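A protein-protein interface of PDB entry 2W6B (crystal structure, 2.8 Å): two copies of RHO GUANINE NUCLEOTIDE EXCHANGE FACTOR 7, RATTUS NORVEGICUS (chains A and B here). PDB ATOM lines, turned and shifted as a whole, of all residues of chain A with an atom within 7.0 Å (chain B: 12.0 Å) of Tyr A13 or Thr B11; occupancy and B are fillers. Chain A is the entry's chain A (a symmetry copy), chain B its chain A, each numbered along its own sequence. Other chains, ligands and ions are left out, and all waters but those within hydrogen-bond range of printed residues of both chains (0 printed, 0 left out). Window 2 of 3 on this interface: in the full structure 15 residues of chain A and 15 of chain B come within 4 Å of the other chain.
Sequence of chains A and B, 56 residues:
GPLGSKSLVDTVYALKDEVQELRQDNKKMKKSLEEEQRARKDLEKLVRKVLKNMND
Tyr A13 touches Thr B11.
CD1 of Leu B15 touches CB of Leu A15, 3.6 Å away.
Leu B15 touches Lys A16.
CG1 of Val A19 touches OE1 of Glu B18, at 3.4 Å.
CG2 of Val A19 touches CG2 of Val B19, 3.5 Å away.
No residue of chain B comes within 4 Å of Val A9.
No residue of chain B comes within 4 Å of Asp A10.
Thr A11 touches none of the printed residues of chain B.
No residue of chain B comes within 4 Å of Ala A14.
Leu A15 touches one residue of chain B.
No residue of chain B comes within 4 Å of Asp A17.
Printed residues of chain B within 4 Å of Val A19: Glu B18 (3.4 Å) and Val B19 (3.5 Å).
Of chain A, only Tyr A13 comes within 4 Å of Thr B11.
Printed residues of chain A within 4 Å of Leu B15: Leu A15 and Lys A16.
Printed residues of chain A within 4 Å of Val B19: Val A19.
The nearest residue of chain B that does not touch Tyr A13 is Ser B7 (5.3 Å).
Printed residues of chain B that touch a printed residue of chain A: Thr B11, Leu B15, Glu B18 and Val B19.
Hydrophobic or aromatic side chains of chain B that line the printed part of chain A: Leu B15 and Val B19.
Along chain B the printed residues that touch a printed residue of chain A span positions 11 to 19.
Printed residues of chain A that touch a printed residue of chain B: Tyr A13, Leu A15, Lys A16 and Val A19.
Hydrophobic or aromatic side chains of chain A within 4 Å of the printed part of chain B: Tyr A13, Leu A15 and Val A19.
Among the printed residues, no Asp or Glu carboxylate lies within 4 Å of a Lys or Arg side-chain nitrogen of the other chain.
The backbone carbonyl oxygen (O) of Ser B7 lies within hydrogen-bond range of the side-chain hydroxyl (OG1) of Thr B11 (2.7 Å).
Tyr A13 touches Thr B11, but with the chains exchanged Thr A11 does not touch Tyr B13 (11.4 Å).
Leu B15 touches its own counterpart, Leu A15.
Lys A16 touches Leu B15, but with the chains exchanged Leu A15 does not touch Lys B16 (7.5 Å).
Val A19 touches Glu B18, but with the chains exchanged Glu A18 does not touch Val B19 (7.5 Å).
Of the 5 pairs that touch across the chains among the printed residues, 2 have their exchanged pair printed and touching as well.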
ATOM      1  N   LEU A   8      26.374 -12.832  -9.861  1.00  0.00           N
ATOM      2  CA  LEU A   8      26.564 -12.700 -11.316  1.00  0.00           C
ATOM      3  C   LEU A   8      25.607 -11.665 -11.908  1.00  0.00           C
ATOM      4  O   LEU A   8      26.016 -10.817 -12.685  1.00  0.00           O
ATOM      5  CB  LEU A   8      26.368 -14.065 -12.003  1.00  0.00           C
ATOM      6  CG  LEU A   8      26.315 -14.302 -13.524  1.00  0.00           C
ATOM      7  CD1 LEU A   8      27.550 -13.767 -14.239  1.00  0.00           C
ATOM      8  CD2 LEU A   8      26.107 -15.803 -13.818  1.00  0.00           C
ATOM      9  N   VAL A   9      24.338 -11.738 -11.519  1.00  0.00           N
ATOM     10  CA  VAL A   9      23.320 -10.794 -11.977  1.00  0.00           C
ATOM     11  C   VAL A   9      23.526  -9.403 -11.367  1.00  0.00           C
ATOM     12  O   VAL A   9      23.237  -8.375 -11.998  1.00  0.00           O
ATOM     13  CB  VAL A   9      21.895 -11.295 -11.628  1.00  0.00           C
ATOM     14  CG1 VAL A   9      20.850 -10.215 -11.909  1.00  0.00           C
ATOM     15  CG2 VAL A   9      21.552 -12.596 -12.387  1.00  0.00           C
ATOM     16  N   ASP A  10      24.022  -9.379 -10.133  1.00  0.00           N
ATOM     17  CA  ASP A  10      24.256  -8.132  -9.423  1.00  0.00           C
ATOM     18  C   ASP A  10      25.262  -7.286 -10.170  1.00  0.00           C
ATOM     19  O   ASP A  10      24.957  -6.163 -10.565  1.00  0.00           O
ATOM     20  CB  ASP A  10      24.755  -8.401  -8.000  1.00  0.00           C
ATOM     21  N   THR A  11      26.452  -7.842 -10.379  1.00  0.00           N
ATOM     22  CA  THR A  11      27.532  -7.114 -11.038  1.00  0.00           C
ATOM     23  C   THR A  11      27.123  -6.564 -12.405  1.00  0.00           C
ATOM     24  O   THR A  11      27.537  -5.470 -12.761  1.00  0.00           O
ATOM     25  CB  THR A  11      28.857  -7.924 -11.098  1.00  0.00           C
ATOM     26  OG1 THR A  11      28.581  -9.301 -10.842  1.00  0.00           O
ATOM     27  CG2 THR A  11      29.840  -7.441 -10.026  1.00  0.00           C
ATOM     28  N   VAL A  12      26.291  -7.292 -13.146  1.00  0.00           N
ATOM     29  CA  VAL A  12      25.838  -6.808 -14.448  1.00  0.00           C
ATOM     30  C   VAL A  12      24.992  -5.559 -14.314  1.00  0.00           C
ATOM     31  O   VAL A  12      25.226  -4.564 -15.002  1.00  0.00           O
ATOM     32  CB  VAL A  12      25.005  -7.832 -15.204  1.00  0.00           C
ATOM     33  CG1 VAL A  12      24.919  -7.447 -16.658  1.00  0.00           C
ATOM     34  CG2 VAL A  12      25.618  -9.193 -15.080  1.00  0.00           C
ATOM     35  N   TYR A  13      24.000  -5.606 -13.433  1.00  0.00           N
ATOM     36  CA  TYR A  13      23.147  -4.444 -13.221  1.00  0.00           C
ATOM     37  C   TYR A  13      23.894  -3.335 -12.501  1.00  0.00           C
ATOM     38  O   TYR A  13      23.633  -2.162 -12.729  1.00  0.00           O
ATOM     39  CB  TYR A  13      21.825  -4.844 -12.563  1.00  0.00           C
ATOM     40  CG  TYR A  13      20.880  -5.427 -13.603  1.00  0.00           C
ATOM     41  CD1 TYR A  13      21.101  -6.702 -14.137  1.00  0.00           C
ATOM     42  CD2 TYR A  13      19.799  -4.684 -14.093  1.00  0.00           C
ATOM     43  CE1 TYR A  13      20.258  -7.238 -15.121  1.00  0.00           C
ATOM     44  CE2 TYR A  13      18.948  -5.205 -15.073  1.00  0.00           C
ATOM     45  CZ  TYR A  13      19.183  -6.488 -15.588  1.00  0.00           C
ATOM     46  OH  TYR A  13      18.353  -7.022 -16.570  1.00  0.00           O
ATOM     47  N   ALA A  14      24.863  -3.718 -11.675  1.00  0.00           N
ATOM     48  CA  ALA A  14      25.825  -2.780 -11.119  1.00  0.00           C
ATOM     49  C   ALA A  14      26.552  -2.073 -12.244  1.00  0.00           C
ATOM     50  O   ALA A  14      26.907  -0.911 -12.115  1.00  0.00           O
ATOM     51  CB  ALA A  14      26.816  -3.507 -10.259  1.00  0.00           C
ATOM     52  N   LEU A  15      26.773  -2.788 -13.346  1.00  0.00           N
ATOM     53  CA  LEU A  15      27.463  -2.246 -14.512  1.00  0.00           C
ATOM     54  C   LEU A  15      26.549  -1.433 -15.384  1.00  0.00           C
ATOM     55  O   LEU A  15      26.995  -0.467 -15.993  1.00  0.00           O
ATOM     56  CB  LEU A  15      28.036  -3.348 -15.384  1.00  0.00           C
ATOM     57  CG  LEU A  15      29.433  -3.935 -15.250  1.00  0.00           C
ATOM     58  CD1 LEU A  15      29.833  -4.340 -16.641  1.00  0.00           C
ATOM     59  CD2 LEU A  15      30.448  -2.973 -14.702  1.00  0.00           C
ATOM     60  N   LYS A  16      25.285  -1.840 -15.490  1.00  0.00           N
ATOM     61  CA  LYS A  16      24.325  -1.058 -16.266  1.00  0.00           C
ATOM     62  C   LYS A  16      24.220   0.331 -15.641  1.00  0.00           C
ATOM     63  O   LYS A  16      24.167   1.336 -16.353  1.00  0.00           O
ATOM     64  CB  LYS A  16      22.954  -1.738 -16.332  1.00  0.00           C
ATOM     65  N   ASP A  17      24.222   0.372 -14.307  1.00  0.00           N
ATOM     66  CA  ASP A  17      24.235   1.622 -13.547  1.00  0.00           C
ATOM     67  C   ASP A  17      25.409   2.476 -13.967  1.00  0.00           C
ATOM     68  O   ASP A  17      25.223   3.548 -14.535  1.00  0.00           O
ATOM     69  CB  ASP A  17      24.315   1.341 -12.036  1.00  0.00           C
ATOM     70  CG  ASP A  17      22.949   1.423 -11.347  1.00  0.00           C
ATOM     71  OD1 ASP A  17      22.480   0.383 -10.790  1.00  0.00           O
ATOM     72  OD2 ASP A  17      22.352   2.538 -11.366  1.00  0.00           O
ATOM     73  N   GLU A  18      26.612   1.967 -13.696  1.00  0.00           N
ATOM     74  CA  GLU A  18      27.871   2.634 -14.011  1.00  0.00           C
ATOM     75  C   GLU A  18      27.929   3.137 -15.432  1.00  0.00           C
ATOM     76  O   GLU A  18      28.403   4.240 -15.670  1.00  0.00           O
ATOM     77  CB  GLU A  18      29.041   1.689 -13.817  1.00  0.00           C
ATOM     78  CG  GLU A  18      29.341   1.321 -12.394  1.00  0.00           C
ATOM     79  CD  GLU A  18      30.606   0.478 -12.290  1.00  0.00           C
ATOM     80  OE1 GLU A  18      31.616   0.838 -12.958  1.00  0.00           O
ATOM     81  OE2 GLU A  18      30.587  -0.537 -11.547  1.00  0.00           O
ATOM     82  N   VAL A  19      27.468   2.326 -16.378  1.00  0.00           N
ATOM     83  CA  VAL A  19      27.454   2.740 -17.772  1.00  0.00           C
ATOM     84  C   VAL A  19      26.454   3.887 -18.022  1.00  0.00           C
ATOM     85  O   VAL A  19      26.791   4.855 -18.712  1.00  0.00           O
ATOM     86  CB  VAL A  19      27.262   1.537 -18.710  1.00  0.00           C
ATOM     87  CG1 VAL A  19      26.722   1.961 -20.060  1.00  0.00           C
ATOM     88  CG2 VAL A  19      28.572   0.810 -18.869  1.00  0.00           C
ATOM     89  N   SER B   5      22.108 -18.243 -19.804  1.00  0.00           N
ATOM     90  CA  SER B   5      20.711 -17.710 -19.719  1.00  0.00           C
ATOM     91  C   SER B   5      20.456 -16.612 -20.749  1.00  0.00           C
ATOM     92  O   SER B   5      21.155 -15.596 -20.760  1.00  0.00           O
ATOM     93  CB  SER B   5      20.398 -17.185 -18.310  1.00  0.00           C
ATOM     94  OG  SER B   5      19.233 -16.362 -18.321  1.00  0.00           O
ATOM     95  N   LYS B   6      19.427 -16.817 -21.572  1.00  0.00           N
ATOM     96  CA  LYS B   6      19.095 -15.938 -22.699  1.00  0.00           C
ATOM     97  C   LYS B   6      19.112 -14.435 -22.367  1.00  0.00           C
ATOM     98  O   LYS B   6      19.939 -13.689 -22.906  1.00  0.00           O
ATOM     99  CB  LYS B   6      17.741 -16.340 -23.297  1.00  0.00           C
ATOM    100  N   SER B   7      18.207 -14.006 -21.484  1.00  0.00           N
ATOM    101  CA  SER B   7      18.104 -12.602 -21.069  1.00  0.00           C
ATOM    102  C   SER B   7      19.348 -12.096 -20.316  1.00  0.00           C
ATOM    103  O   SER B   7      19.790 -10.971 -20.549  1.00  0.00           O
ATOM    104  CB  SER B   7      16.844 -12.388 -20.233  1.00  0.00           C
ATOM    105  OG  SER B   7      16.994 -11.267 -19.387  1.00  0.00           O
ATOM    106  N   LEU B   8      19.890 -12.925 -19.416  1.00  0.00           N
ATOM    107  CA  LEU B   8      21.163 -12.651 -18.725  1.00  0.00           C
ATOM    108  C   LEU B   8      22.288 -12.381 -19.724  1.00  0.00           C
ATOM    109  O   LEU B   8      23.037 -11.430 -19.570  1.00  0.00           O
ATOM    110  CB  LEU B   8      21.532 -13.832 -17.808  1.00  0.00           C
ATOM    111  CG  LEU B   8      22.867 -13.997 -17.056  1.00  0.00           C
ATOM    112  CD1 LEU B   8      23.186 -12.800 -16.168  1.00  0.00           C
ATOM    113  CD2 LEU B   8      22.856 -15.308 -16.242  1.00  0.00           C
ATOM    114  N   VAL B   9      22.383 -13.218 -20.752  1.00  0.00           N
ATOM    115  CA  VAL B   9      23.389 -13.062 -21.802  1.00  0.00           C
ATOM    116  C   VAL B   9      23.089 -11.851 -22.693  1.00  0.00           C
ATOM    117  O   VAL B   9      24.005 -11.182 -23.197  1.00  0.00           O
ATOM    118  CB  VAL B   9      23.476 -14.333 -22.685  1.00  0.00           C
ATOM    119  CG1 VAL B   9      24.365 -14.091 -23.907  1.00  0.00           C
ATOM    120  CG2 VAL B   9      23.981 -15.548 -21.877  1.00  0.00           C
ATOM    121  N   ASP B  10      21.803 -11.579 -22.887  1.00  0.00           N
ATOM    122  CA  ASP B  10      21.369 -10.470 -23.722  1.00  0.00           C
ATOM    123  C   ASP B  10      21.873  -9.161 -23.156  1.00  0.00           C
ATOM    124  O   ASP B  10      22.604  -8.435 -23.826  1.00  0.00           O
ATOM    125  CB  ASP B  10      19.842 -10.435 -23.833  1.00  0.00           C
ATOM    126  N   THR B  11      21.497  -8.880 -21.911  1.00  0.00           N
ATOM    127  CA  THR B  11      21.867  -7.625 -21.265  1.00  0.00           C
ATOM    128  C   THR B  11      23.377  -7.382 -21.271  1.00  0.00           C
ATOM    129  O   THR B  11      23.804  -6.247 -21.431  1.00  0.00           O
ATOM    130  CB  THR B  11      21.247  -7.470 -19.849  1.00  0.00           C
ATOM    131  OG1 THR B  11      20.795  -8.744 -19.389  1.00  0.00           O
ATOM    132  CG2 THR B  11      20.036  -6.532 -19.882  1.00  0.00           C
ATOM    133  N   VAL B  12      24.178  -8.437 -21.136  1.00  0.00           N
ATOM    134  CA  VAL B  12      25.630  -8.276 -21.163  1.00  0.00           C
ATOM    135  C   VAL B  12      26.110  -7.794 -22.517  1.00  0.00           C
ATOM    136  O   VAL B  12      26.878  -6.835 -22.607  1.00  0.00           O
ATOM    137  CB  VAL B  12      26.375  -9.566 -20.859  1.00  0.00           C
ATOM    138  CG1 VAL B  12      27.807  -9.258 -20.505  1.00  0.00           C
ATOM    139  CG2 VAL B  12      25.721 -10.287 -19.720  1.00  0.00           C
ATOM    140  N   TYR B  13      25.668  -8.462 -23.575  1.00  0.00           N
ATOM    141  CA  TYR B  13      26.060  -8.057 -24.919  1.00  0.00           C
ATOM    142  C   TYR B  13      25.399  -6.750 -25.316  1.00  0.00           C
ATOM    143  O   TYR B  13      25.975  -5.964 -26.056  1.00  0.00           O
ATOM    144  CB  TYR B  13      25.856  -9.196 -25.919  1.00  0.00           C
ATOM    145  CG  TYR B  13      27.001 -10.193 -25.816  1.00  0.00           C
ATOM    146  CD1 TYR B  13      27.103 -11.056 -24.719  1.00  0.00           C
ATOM    147  CD2 TYR B  13      28.012 -10.233 -26.784  1.00  0.00           C
ATOM    148  CE1 TYR B  13      28.172 -11.955 -24.594  1.00  0.00           C
ATOM    149  CE2 TYR B  13      29.085 -11.126 -26.675  1.00  0.00           C
ATOM    150  CZ  TYR B  13      29.162 -11.989 -25.573  1.00  0.00           C
ATOM    151  OH  TYR B  13      30.223 -12.878 -25.440  1.00  0.00           O
ATOM    152  N   ALA B  14      24.211  -6.501 -24.773  1.00  0.00           N
ATOM    153  CA  ALA B  14      23.579  -5.194 -24.852  1.00  0.00           C
ATOM    154  C   ALA B  14      24.493  -4.151 -24.243  1.00  0.00           C
ATOM    155  O   ALA B  14      24.519  -3.016 -24.694  1.00  0.00           O
ATOM    156  CB  ALA B  14      22.271  -5.209 -24.116  1.00  0.00           C
ATOM    157  N   LEU B  15      25.238  -4.548 -23.212  1.00  0.00           N
ATOM    158  CA  LEU B  15      26.163  -3.657 -22.521  1.00  0.00           C
ATOM    159  C   LEU B  15      27.473  -3.528 -23.244  1.00  0.00           C
ATOM    160  O   LEU B  15      28.085  -2.466 -23.202  1.00  0.00           O
ATOM    161  CB  LEU B  15      26.481  -4.159 -21.123  1.00  0.00           C
ATOM    162  CG  LEU B  15      25.714  -3.790 -19.863  1.00  0.00           C
ATOM    163  CD1 LEU B  15      26.726  -3.821 -18.753  1.00  0.00           C
ATOM    164  CD2 LEU B  15      25.075  -2.431 -19.915  1.00  0.00           C
ATOM    165  N   LYS B  16      27.934  -4.610 -23.869  1.00  0.00           N
ATOM    166  CA  LYS B  16      29.168  -4.535 -24.650  1.00  0.00           C
ATOM    167  C   LYS B  16      28.968  -3.515 -25.768  1.00  0.00           C
ATOM    168  O   LYS B  16      29.864  -2.719 -26.057  1.00  0.00           O
ATOM    169  CB  LYS B  16      29.569  -5.902 -25.216  1.00  0.00           C
ATOM    170  N   ASP B  17      27.774  -3.530 -26.366  1.00  0.00           N
ATOM    171  CA  ASP B  17      27.378  -2.553 -27.380  1.00  0.00           C
ATOM    172  C   ASP B  17      27.528  -1.150 -26.840  1.00  0.00           C
ATOM    173  O   ASP B  17      28.359  -0.386 -27.322  1.00  0.00           O
ATOM    174  CB  ASP B  17      25.922  -2.785 -27.820  1.00  0.00           C
ATOM    175  CG  ASP B  17      25.819  -3.568 -29.133  1.00  0.00           C
ATOM    176  OD1 ASP B  17      25.245  -4.700 -29.129  1.00  0.00           O
ATOM    177  OD2 ASP B  17      26.316  -3.038 -30.168  1.00  0.00           O
ATOM    178  N   GLU B  18      26.726  -0.841 -25.820  1.00  0.00           N
ATOM    179  CA  GLU B  18      26.706   0.461 -25.162  1.00  0.00           C
ATOM    180  C   GLU B  18      28.084   0.949 -24.786  1.00  0.00           C
ATOM    181  O   GLU B  18      28.383   2.123 -24.960  1.00  0.00           O
ATOM    182  CB  GLU B  18      25.883   0.405 -23.889  1.00  0.00           C
ATOM    183  CG  GLU B  18      24.404   0.240 -24.087  1.00  0.00           C
ATOM    184  CD  GLU B  18      23.652   0.327 -22.765  1.00  0.00           C
ATOM    185  OE1 GLU B  18      23.969   1.247 -21.960  1.00  0.00           O
ATOM    186  OE2 GLU B  18      22.751  -0.521 -22.535  1.00  0.00           O
ATOM    187  N   VAL B  19      28.914   0.060 -24.253  1.00  0.00           N
ATOM    188  CA  VAL B  19      30.271   0.433 -23.891  1.00  0.00           C
ATOM    189  C   VAL B  19      31.131   0.754 -25.131  1.00  0.00           C
ATOM    190  O   VAL B  19      31.856   1.754 -25.131  1.00  0.00           O
ATOM    191  CB  VAL B  19      30.905  -0.608 -22.953  1.00  0.00           C
ATOM    192  CG1 VAL B  19      32.418  -0.546 -22.988  1.00  0.00           C
ATOM    193  CG2 VAL B  19      30.401  -0.392 -21.550  1.00  0.00           C
ATOM    194  N   GLN B  20      31.028  -0.056 -26.190  1.00  0.00           N
ATOM    195  CA  GLN B  20      31.763   0.203 -27.449  1.00  0.00           C
ATOM    196  C   GLN B  20      31.465   1.603 -28.029  1.00  0.00           C
ATOM    197  O   GLN B  20      32.384   2.342 -28.377  1.00  0.00           O
ATOM    198  CB  GLN B  20      31.479  -0.900 -28.481  1.00  0.00           C
ATOM    199  CG  GLN B  20      32.433  -0.929 -29.699  1.00  0.00           C
ATOM    200  CD  GLN B  20      31.947  -0.092 -30.904  1.00  0.00           C
ATOM    201  OE1 GLN B  20      32.646   0.825 -31.359  1.00  0.00           O
ATOM    202  NE2 GLN B  20      30.757  -0.417 -31.427  1.00  0.00           N
ATOM    203  N   GLU B  21      30.186   1.963 -28.102  1.00  0.00           N
ATOM    204  CA  GLU B  21      29.766   3.277 -28.572  1.00  0.00           C
ATOM    205  C   GLU B  21      30.248   4.390 -27.659  1.00  0.00           C
ATOM    206  O   GLU B  21      30.314   5.533 -28.081  1.00  0.00           O
ATOM    207  CB  GLU B  21      28.244   3.332 -28.714  1.00  0.00           C
ATOM    208  CG  GLU B  21      27.695   2.411 -29.836  1.00  0.00           C
ATOM    209  CD  GLU B  21      26.201   2.037 -29.670  1.00  0.00           C
ATOM    210  OE1 GLU B  21      25.510   2.615 -28.786  1.00  0.00           O
ATOM    211  OE2 GLU B  21      25.719   1.157 -30.436  1.00  0.00           O
